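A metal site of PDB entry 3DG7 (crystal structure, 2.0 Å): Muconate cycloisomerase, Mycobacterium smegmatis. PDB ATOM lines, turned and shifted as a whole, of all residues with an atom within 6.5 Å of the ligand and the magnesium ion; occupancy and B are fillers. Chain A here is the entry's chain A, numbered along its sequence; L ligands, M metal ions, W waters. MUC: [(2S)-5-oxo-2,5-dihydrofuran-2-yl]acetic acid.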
ATOM      1  N   LEU A  19      27.397  15.561  28.627  1.00  0.00           N
ATOM      2  CA  LEU A  19      26.305  14.698  28.197  1.00  0.00           C
ATOM      3  C   LEU A  19      26.571  14.427  26.718  1.00  0.00           C
ATOM      4  O   LEU A  19      26.610  15.351  25.907  1.00  0.00           O
ATOM      5  CB  LEU A  19      24.944  15.389  28.372  1.00  0.00           C
ATOM      6  CG  LEU A  19      23.734  14.513  28.035  1.00  0.00           C
ATOM      7  CD1 LEU A  19      23.642  13.371  29.035  1.00  0.00           C
ATOM      8  CD2 LEU A  19      22.462  15.340  28.027  1.00  0.00           C
ATOM      9  N   PHE A  21      25.647  12.301  23.084  1.00  0.00           N
ATOM     10  CA  PHE A  21      24.598  11.621  22.330  1.00  0.00           C
ATOM     11  C   PHE A  21      24.964  11.590  20.841  1.00  0.00           C
ATOM     12  O   PHE A  21      25.995  12.135  20.442  1.00  0.00           O
ATOM     13  CB  PHE A  21      23.247  12.329  22.567  1.00  0.00           C
ATOM     14  CG  PHE A  21      23.342  13.823  22.594  1.00  0.00           C
ATOM     15  CD1 PHE A  21      23.116  14.570  21.429  1.00  0.00           C
ATOM     16  CD2 PHE A  21      23.683  14.491  23.759  1.00  0.00           C
ATOM     17  CE1 PHE A  21      23.237  15.959  21.441  1.00  0.00           C
ATOM     18  CE2 PHE A  21      23.808  15.883  23.785  1.00  0.00           C
ATOM     19  CZ  PHE A  21      23.589  16.620  22.627  1.00  0.00           C
ATOM     20  N   SER A  23      23.780  13.088  18.000  1.00  0.00           N
ATOM     21  CA  SER A  23      23.897  14.335  17.252  1.00  0.00           C
ATOM     22  C   SER A  23      24.897  15.364  17.784  1.00  0.00           C
ATOM     23  O   SER A  23      25.217  16.330  17.083  1.00  0.00           O
ATOM     24  CB  SER A  23      22.515  14.982  17.112  1.00  0.00           C
ATOM     25  OG  SER A  23      21.935  15.239  18.378  1.00  0.00           O
ATOM     26  N   ARG A  51      21.154  25.057  20.592  1.00  0.00           N
ATOM     27  CA  ARG A  51      21.447  23.689  20.205  1.00  0.00           C
ATOM     28  C   ARG A  51      21.645  23.668  18.690  1.00  0.00           C
ATOM     29  O   ARG A  51      20.737  23.334  17.932  1.00  0.00           O
ATOM     30  CB  ARG A  51      20.301  22.764  20.622  1.00  0.00           C
ATOM     31  CG  ARG A  51      20.019  22.767  22.126  1.00  0.00           C
ATOM     32  CD  ARG A  51      21.132  22.093  22.913  1.00  0.00           C
ATOM     33  NE  ARG A  51      20.931  22.168  24.361  1.00  0.00           N
ATOM     34  CZ  ARG A  51      21.593  22.991  25.177  1.00  0.00           C
ATOM     35  NH1 ARG A  51      22.501  23.823  24.693  1.00  0.00           N
ATOM     36  NH2 ARG A  51      21.361  22.948  26.488  1.00  0.00           N
ATOM     37  N   PHE A  53      23.114  21.656  16.778  1.00  0.00           N
ATOM     38  CA  PHE A  53      22.905  20.324  16.228  1.00  0.00           C
ATOM     39  C   PHE A  53      21.443  19.886  16.265  1.00  0.00           C
ATOM     40  O   PHE A  53      21.119  18.759  15.893  1.00  0.00           O
ATOM     41  CB  PHE A  53      23.771  19.339  17.004  1.00  0.00           C
ATOM     42  CG  PHE A  53      23.698  19.522  18.495  1.00  0.00           C
ATOM     43  CD1 PHE A  53      22.517  19.255  19.191  1.00  0.00           C
ATOM     44  CD2 PHE A  53      24.807  19.986  19.209  1.00  0.00           C
ATOM     45  CE1 PHE A  53      22.448  19.447  20.577  1.00  0.00           C
ATOM     46  CE2 PHE A  53      24.746  20.188  20.590  1.00  0.00           C
ATOM     47  CZ  PHE A  53      23.560  19.918  21.273  1.00  0.00           C
ATOM     48  N   THR A  54      20.551  20.772  16.728  1.00  0.00           N
ATOM     49  CA  THR A  54      19.128  20.461  16.821  1.00  0.00           C
ATOM     50  C   THR A  54      18.266  21.488  16.094  1.00  0.00           C
ATOM     51  O   THR A  54      17.377  21.118  15.315  1.00  0.00           O
ATOM     52  CB  THR A  54      18.657  20.375  18.300  1.00  0.00           C
ATOM     53  OG1 THR A  54      19.406  19.364  18.979  1.00  0.00           O
ATOM     54  CG2 THR A  54      17.174  20.013  18.373  1.00  0.00           C
ATOM     55  N   TYR A  55      18.518  22.770  16.339  1.00  0.00           N
ATOM     56  CA  TYR A  55      17.754  23.846  15.704  1.00  0.00           C
ATOM     57  C   TYR A  55      18.639  24.801  14.904  1.00  0.00           C
ATOM     58  O   TYR A  55      18.138  25.620  14.141  1.00  0.00           O
ATOM     59  CB  TYR A  55      16.993  24.668  16.753  1.00  0.00           C
ATOM     60  CG  TYR A  55      16.155  23.835  17.683  1.00  0.00           C
ATOM     61  CD1 TYR A  55      15.102  23.057  17.195  1.00  0.00           C
ATOM     62  CD2 TYR A  55      16.408  23.814  19.057  1.00  0.00           C
ATOM     63  CE1 TYR A  55      14.328  22.279  18.050  1.00  0.00           C
ATOM     64  CE2 TYR A  55      15.646  23.049  19.919  1.00  0.00           C
ATOM     65  CZ  TYR A  55      14.604  22.272  19.411  1.00  0.00           C
ATOM     66  OH  TYR A  55      13.847  21.501  20.250  1.00  0.00           O
ATOM     67  N   MET A 134      17.636  10.984  31.299  1.00  0.00           N
ATOM     68  CA  MET A 134      18.294  10.632  30.043  1.00  0.00           C
ATOM     69  C   MET A 134      19.732  10.179  30.300  1.00  0.00           C
ATOM     70  O   MET A 134      20.527  10.939  30.865  1.00  0.00           O
ATOM     71  CB  MET A 134      18.314  11.821  29.081  1.00  0.00           C
ATOM     72  CG  MET A 134      16.968  12.495  28.860  1.00  0.00           C
ATOM     73  SD  MET A 134      16.955  13.689  27.492  1.00  0.00           S
ATOM     74  CE  MET A 134      18.025  14.977  28.136  1.00  0.00           C
ATOM     75  N   LYS A 160      15.513   7.116  29.908  1.00  0.00           N
ATOM     76  CA  LYS A 160      15.537   7.162  28.442  1.00  0.00           C
ATOM     77  C   LYS A 160      17.003   6.963  28.063  1.00  0.00           C
ATOM     78  O   LYS A 160      17.832   7.832  28.318  1.00  0.00           O
ATOM     79  CB  LYS A 160      15.033   8.503  27.901  1.00  0.00           C
ATOM     80  CG  LYS A 160      15.074   8.564  26.378  1.00  0.00           C
ATOM     81  CD  LYS A 160      14.353   9.770  25.811  1.00  0.00           C
ATOM     82  CE  LYS A 160      15.219  11.019  25.806  1.00  0.00           C
ATOM     83  NZ  LYS A 160      14.511  12.110  25.100  1.00  0.00           N
ATOM     84  N   LYS A 162      20.162   6.870  25.693  1.00  0.00           N
ATOM     85  CA  LYS A 162      20.656   7.458  24.454  1.00  0.00           C
ATOM     86  C   LYS A 162      21.323   6.346  23.657  1.00  0.00           C
ATOM     87  O   LYS A 162      22.185   5.634  24.168  1.00  0.00           O
ATOM     88  CB  LYS A 162      21.685   8.550  24.744  1.00  0.00           C
ATOM     89  CG  LYS A 162      21.124   9.841  25.303  1.00  0.00           C
ATOM     90  CD  LYS A 162      20.258  10.537  24.264  1.00  0.00           C
ATOM     91  CE  LYS A 162      19.793  11.888  24.766  1.00  0.00           C
ATOM     92  NZ  LYS A 162      19.069  12.613  23.698  1.00  0.00           N
ATOM     93  N   ASP A 191      16.332   6.789  22.662  1.00  0.00           N
ATOM     94  CA  ASP A 191      16.399   7.967  21.802  1.00  0.00           C
ATOM     95  C   ASP A 191      17.715   7.854  21.016  1.00  0.00           C
ATOM     96  O   ASP A 191      18.795   7.897  21.596  1.00  0.00           O
ATOM     97  CB  ASP A 191      16.388   9.237  22.658  1.00  0.00           C
ATOM     98  CG  ASP A 191      16.243  10.502  21.847  1.00  0.00           C
ATOM     99  OD1 ASP A 191      16.586  10.484  20.642  1.00  0.00           O
ATOM    100  OD2 ASP A 191      15.799  11.528  22.412  1.00  0.00           O
ATOM    101  N   ASN A 193      18.643   9.938  18.465  1.00  0.00           N
ATOM    102  CA  ASN A 193      19.059  11.228  17.928  1.00  0.00           C
ATOM    103  C   ASN A 193      19.542  11.171  16.471  1.00  0.00           C
ATOM    104  O   ASN A 193      20.577  11.742  16.127  1.00  0.00           O
ATOM    105  CB  ASN A 193      20.143  11.862  18.811  1.00  0.00           C
ATOM    106  CG  ASN A 193      19.578  12.422  20.098  1.00  0.00           C
ATOM    107  OD1 ASN A 193      19.878  11.941  21.195  1.00  0.00           O
ATOM    108  ND2 ASN A 193      18.743  13.447  19.974  1.00  0.00           N
ATOM    109  N   GLU A 217      12.522   6.775  20.149  1.00  0.00           N
ATOM    110  CA  GLU A 217      12.580   8.190  19.791  1.00  0.00           C
ATOM    111  C   GLU A 217      13.673   8.531  18.793  1.00  0.00           C
ATOM    112  O   GLU A 217      14.849   8.229  19.018  1.00  0.00           O
ATOM    113  CB  GLU A 217      12.777   9.040  21.066  1.00  0.00           C
ATOM    114  CG  GLU A 217      12.733  10.545  20.833  1.00  0.00           C
ATOM    115  CD  GLU A 217      12.683  11.338  22.129  1.00  0.00           C
ATOM    116  OE1 GLU A 217      12.146  10.791  23.126  1.00  0.00           O
ATOM    117  OE2 GLU A 217      13.141  12.498  22.157  1.00  0.00           O
ATOM    118  N   GLU A 218      13.274   9.148  17.677  1.00  0.00           N
ATOM    119  CA  GLU A 218      14.196   9.565  16.623  1.00  0.00           C
ATOM    120  C   GLU A 218      15.363   8.602  16.385  1.00  0.00           C
ATOM    121  O   GLU A 218      16.519   9.021  16.374  1.00  0.00           O
ATOM    122  CB  GLU A 218      14.747  10.960  16.954  1.00  0.00           C
ATOM    123  CG  GLU A 218      13.698  12.075  17.010  1.00  0.00           C
ATOM    124  CD  GLU A 218      13.183  12.482  15.641  1.00  0.00           C
ATOM    125  OE1 GLU A 218      13.680  11.932  14.638  1.00  0.00           O
ATOM    126  OE2 GLU A 218      12.296  13.349  15.565  1.00  0.00           O
ATOM    127  N   ILE A 240       8.394   8.311  18.892  1.00  0.00           N
ATOM    128  CA  ILE A 240       8.426   9.722  19.234  1.00  0.00           C
ATOM    129  C   ILE A 240       9.257  10.596  18.296  1.00  0.00           C
ATOM    130  O   ILE A 240      10.436  10.329  18.079  1.00  0.00           O
ATOM    131  CB  ILE A 240       8.983   9.948  20.659  1.00  0.00           C
ATOM    132  CG1 ILE A 240       8.103   9.231  21.693  1.00  0.00           C
ATOM    133  CG2 ILE A 240       9.048  11.449  20.966  1.00  0.00           C
ATOM    134  CD1 ILE A 240       8.631   9.317  23.124  1.00  0.00           C
ATOM    135  N   ASP A 242      10.906  14.197  17.739  1.00  0.00           N
ATOM    136  CA  ASP A 242      11.424  15.239  18.624  1.00  0.00           C
ATOM    137  C   ASP A 242      11.980  16.391  17.798  1.00  0.00           C
ATOM    138  O   ASP A 242      11.259  17.351  17.484  1.00  0.00           O
ATOM    139  CB  ASP A 242      12.508  14.632  19.530  1.00  0.00           C
ATOM    140  CG  ASP A 242      13.185  15.653  20.446  1.00  0.00           C
ATOM    141  OD1 ASP A 242      12.829  16.843  20.405  1.00  0.00           O
ATOM    142  OD2 ASP A 242      14.087  15.247  21.201  1.00  0.00           O
ATOM    143  N   GLU A 243      13.252  16.305  17.417  1.00  0.00           N
ATOM    144  CA  GLU A 243      13.852  17.376  16.633  1.00  0.00           C
ATOM    145  C   GLU A 243      13.179  17.588  15.268  1.00  0.00           C
ATOM    146  O   GLU A 243      13.307  18.652  14.669  1.00  0.00           O
ATOM    147  CB  GLU A 243      15.349  17.133  16.438  1.00  0.00           C
ATOM    148  CG  GLU A 243      15.734  15.751  15.943  1.00  0.00           C
ATOM    149  CD  GLU A 243      16.203  14.845  17.080  1.00  0.00           C
ATOM    150  OE1 GLU A 243      17.292  14.249  16.937  1.00  0.00           O
ATOM    151  OE2 GLU A 243      15.480  14.738  18.093  1.00  0.00           O
ATOM    152  N   SER A 264       6.972  14.545  20.992  1.00  0.00           N
ATOM    153  CA  SER A 264       7.735  15.080  22.095  1.00  0.00           C
ATOM    154  C   SER A 264       7.390  16.560  22.211  1.00  0.00           C
ATOM    155  O   SER A 264       7.357  17.283  21.213  1.00  0.00           O
ATOM    156  CB  SER A 264       9.232  14.929  21.816  1.00  0.00           C
ATOM    157  OG  SER A 264       9.998  15.827  22.614  1.00  0.00           O
ATOM    158  N   LYS A 266       8.626  19.995  24.036  1.00  0.00           N
ATOM    159  CA  LYS A 266       9.707  20.601  24.811  1.00  0.00           C
ATOM    160  C   LYS A 266       9.443  22.082  24.921  1.00  0.00           C
ATOM    161  O   LYS A 266       9.389  22.798  23.916  1.00  0.00           O
ATOM    162  CB  LYS A 266      11.064  20.346  24.130  1.00  0.00           C
ATOM    163  CG  LYS A 266      11.496  18.877  24.164  1.00  0.00           C
ATOM    164  CD  LYS A 266      12.911  18.693  23.630  1.00  0.00           C
ATOM    165  CE  LYS A 266      13.327  17.242  23.635  1.00  0.00           C
ATOM    166  NZ  LYS A 266      14.768  17.089  23.270  1.00  0.00           N
ATOM    167  N   GLY A 292       9.689  16.397  26.906  1.00  0.00           N
ATOM    168  CA  GLY A 292      11.097  16.096  26.727  1.00  0.00           C
ATOM    169  C   GLY A 292      12.031  17.089  27.385  1.00  0.00           C
ATOM    170  O   GLY A 292      11.595  18.116  27.909  1.00  0.00           O
ATOM    171  N   ASN A 293      13.321  16.781  27.346  1.00  0.00           N
ATOM    172  CA  ASN A 293      14.360  17.613  27.950  1.00  0.00           C
ATOM    173  C   ASN A 293      15.291  18.111  26.842  1.00  0.00           C
ATOM    174  O   ASN A 293      15.757  17.323  26.025  1.00  0.00           O
ATOM    175  CB  ASN A 293      15.135  16.799  28.981  1.00  0.00           C
ATOM    176  CG  ASN A 293      16.029  17.660  29.864  1.00  0.00           C
ATOM    177  OD1 ASN A 293      17.028  18.210  29.407  1.00  0.00           O
ATOM    178  ND2 ASN A 293      15.671  17.770  31.146  1.00  0.00           N
ATOM    179  N   GLN A 294      15.547  19.415  26.824  1.00  0.00           N
ATOM    180  CA  GLN A 294      16.429  20.020  25.825  1.00  0.00           C
ATOM    181  C   GLN A 294      17.824  20.187  26.443  1.00  0.00           C
ATOM    182  O   GLN A 294      18.604  21.046  26.022  1.00  0.00           O
ATOM    183  CB  GLN A 294      15.865  21.401  25.451  1.00  0.00           C
ATOM    184  CG  GLN A 294      16.348  21.948  24.118  1.00  0.00           C
ATOM    185  CD  GLN A 294      15.584  21.347  22.946  1.00  0.00           C
ATOM    186  OE1 GLN A 294      14.453  21.728  22.662  1.00  0.00           O
ATOM    187  NE2 GLN A 294      16.211  20.395  22.280  1.00  0.00           N
ATOM    188  N   ILE A 295      18.135  19.328  27.418  1.00  0.00           N
ATOM    189  CA  ILE A 295      19.383  19.393  28.177  1.00  0.00           C
ATOM    190  C   ILE A 295      19.276  20.731  28.889  1.00  0.00           C
ATOM    191  O   ILE A 295      20.191  21.564  28.874  1.00  0.00           O
ATOM    192  CB  ILE A 295      20.635  19.365  27.271  1.00  0.00           C
ATOM    193  CG1 ILE A 295      20.565  18.176  26.302  1.00  0.00           C
ATOM    194  CG2 ILE A 295      21.879  19.190  28.144  1.00  0.00           C
ATOM    195  CD1 ILE A 295      21.704  18.128  25.303  1.00  0.00           C
ATOM    196  N   GLU A 320      10.882  14.285  31.261  1.00  0.00           N
ATOM    197  CA  GLU A 320      12.343  14.311  31.293  1.00  0.00           C
ATOM    198  C   GLU A 320      12.745  15.602  32.014  1.00  0.00           C
ATOM    199  O   GLU A 320      12.910  16.663  31.409  1.00  0.00           O
ATOM    200  CB  GLU A 320      12.865  14.250  29.854  1.00  0.00           C
ATOM    201  CG  GLU A 320      12.696  12.845  29.283  1.00  0.00           C
ATOM    202  CD  GLU A 320      12.631  12.802  27.755  1.00  0.00           C
ATOM    203  OE1 GLU A 320      13.313  13.608  27.091  1.00  0.00           O
ATOM    204  OE2 GLU A 320      11.894  11.932  27.234  1.00  0.00           O
HETATM  205  C1  MUC L   1      16.577  14.576  23.225  1.00  0.00           C
HETATM  206  O1  MUC L   1      15.458  14.199  23.661  1.00  0.00           O
HETATM  207  O2  MUC L   1      16.940  14.535  22.025  1.00  0.00           O
HETATM  208  C4  MUC L   1      19.588  15.811  22.729  1.00  0.00           C
HETATM  209  C5  MUC L   1      19.779  16.934  22.022  1.00  0.00           C
HETATM  210  C6  MUC L   1      18.866  17.841  22.403  1.00  0.00           C
HETATM  211  O6  MUC L   1      18.873  19.025  22.067  1.00  0.00           O
HETATM  212  O3  MUC L   1      17.909  17.305  23.220  1.00  0.00           O
HETATM  213  C3  MUC L   1      18.580  16.205  23.819  1.00  0.00           C
HETATM  214  C2  MUC L   1      17.591  15.099  24.292  1.00  0.00           C
HETATM  215 MG    MG M   1      14.962  13.315  21.863  1.00  0.00          MG
HETATM  216  O   HOH W   1      15.403  12.903  19.905  1.00  0.00           O
HETATM  217  O   HOH W   2      17.250  16.307  20.003  1.00  0.00           O
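Merely in contact with the ligand: Phe 21, Arg 51, Phe 53, Met 134, Asn 293 and Ile 295.
Of the 24 residues printed, 15 come within 4 Å of the ligand.
The magnesium ion is bound by OE2 of Glu 217 (2.0 Å), OD2 of Asp 191 (2.0 Å), water W1 (2.0 Å), O1 of the ligand (2.1 Å), OD2 of Asp 242 (2.2 Å) and O2 of the ligand (2.3 Å).
The magnesium ion has six donor atoms within binding distance.
NZ of Lys 160 lies close to OD2 of Asp 191, at 3.0 Å.
The backbone NH of Asn 193 is in hydrogen-bond range of the side-chain carboxylate of Asp 191, 3.0 Å away.
OD2 of Asp 191 lies close to NZ of Lys 162, 3.7 Å away.
NZ of Lys 160 is in salt-bridge range of OE1 of Glu 320 (2.8 Å).
OD1 of Asn 193 lies within hydrogen-bond range of NZ of Lys 162.
NZ of Lys 266 lies within hydrogen-bond range of O of Asn 293 (2.9 Å).
ND2 of Asn 293 lies within hydrogen-bond range of O of Glu 320.
The guanidinium group of Arg 51 lies within hydrogen-bond range of the backbone carbonyl oxygen of Ile 295 (3.0 Å).
An oxygen (O1) of the ligand sits close to the side-chain amino group (NZ) of Lys 160.
ND2 of Asn 193 lies close to O2 of the ligand (2.9 Å).
The side-chain amino group (NZ) of Lys 162 lies close to an oxygen (O2) of the ligand.
An oxygen (O3) of the ligand lies close to the side-chain amino group (NZ) of Lys 266.
The side-chain amide nitrogen (NE2) of Gln 294 sits at hydrogen-bond distance from an oxygen (O6) of the ligand (3.0 Å).
OG1 of Thr 54 sits at hydrogen-bond distance from O6 of the ligand (3.2 Å).
Residues that only touch the magnesium ion: Lys 160.
Four residues have an atom within 4 Å of the magnesium ion: Lys 160, Asp 191, Glu 217 and Asp 242.
Water W1 lies within hydrogen-bond range of the side-chain carboxylate of Glu 243 (2.6 Å), the side-chain carboxylate of Asp 191 (2.8 Å) and the side-chain amide nitrogen of Asn 193 (3.4 Å).
Water W2 lies within hydrogen-bond range of OE2 of Glu 243 (3.0 Å), ND2 of Asn 193 (3.2 Å) and O3 of the ligand (3.4 Å).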
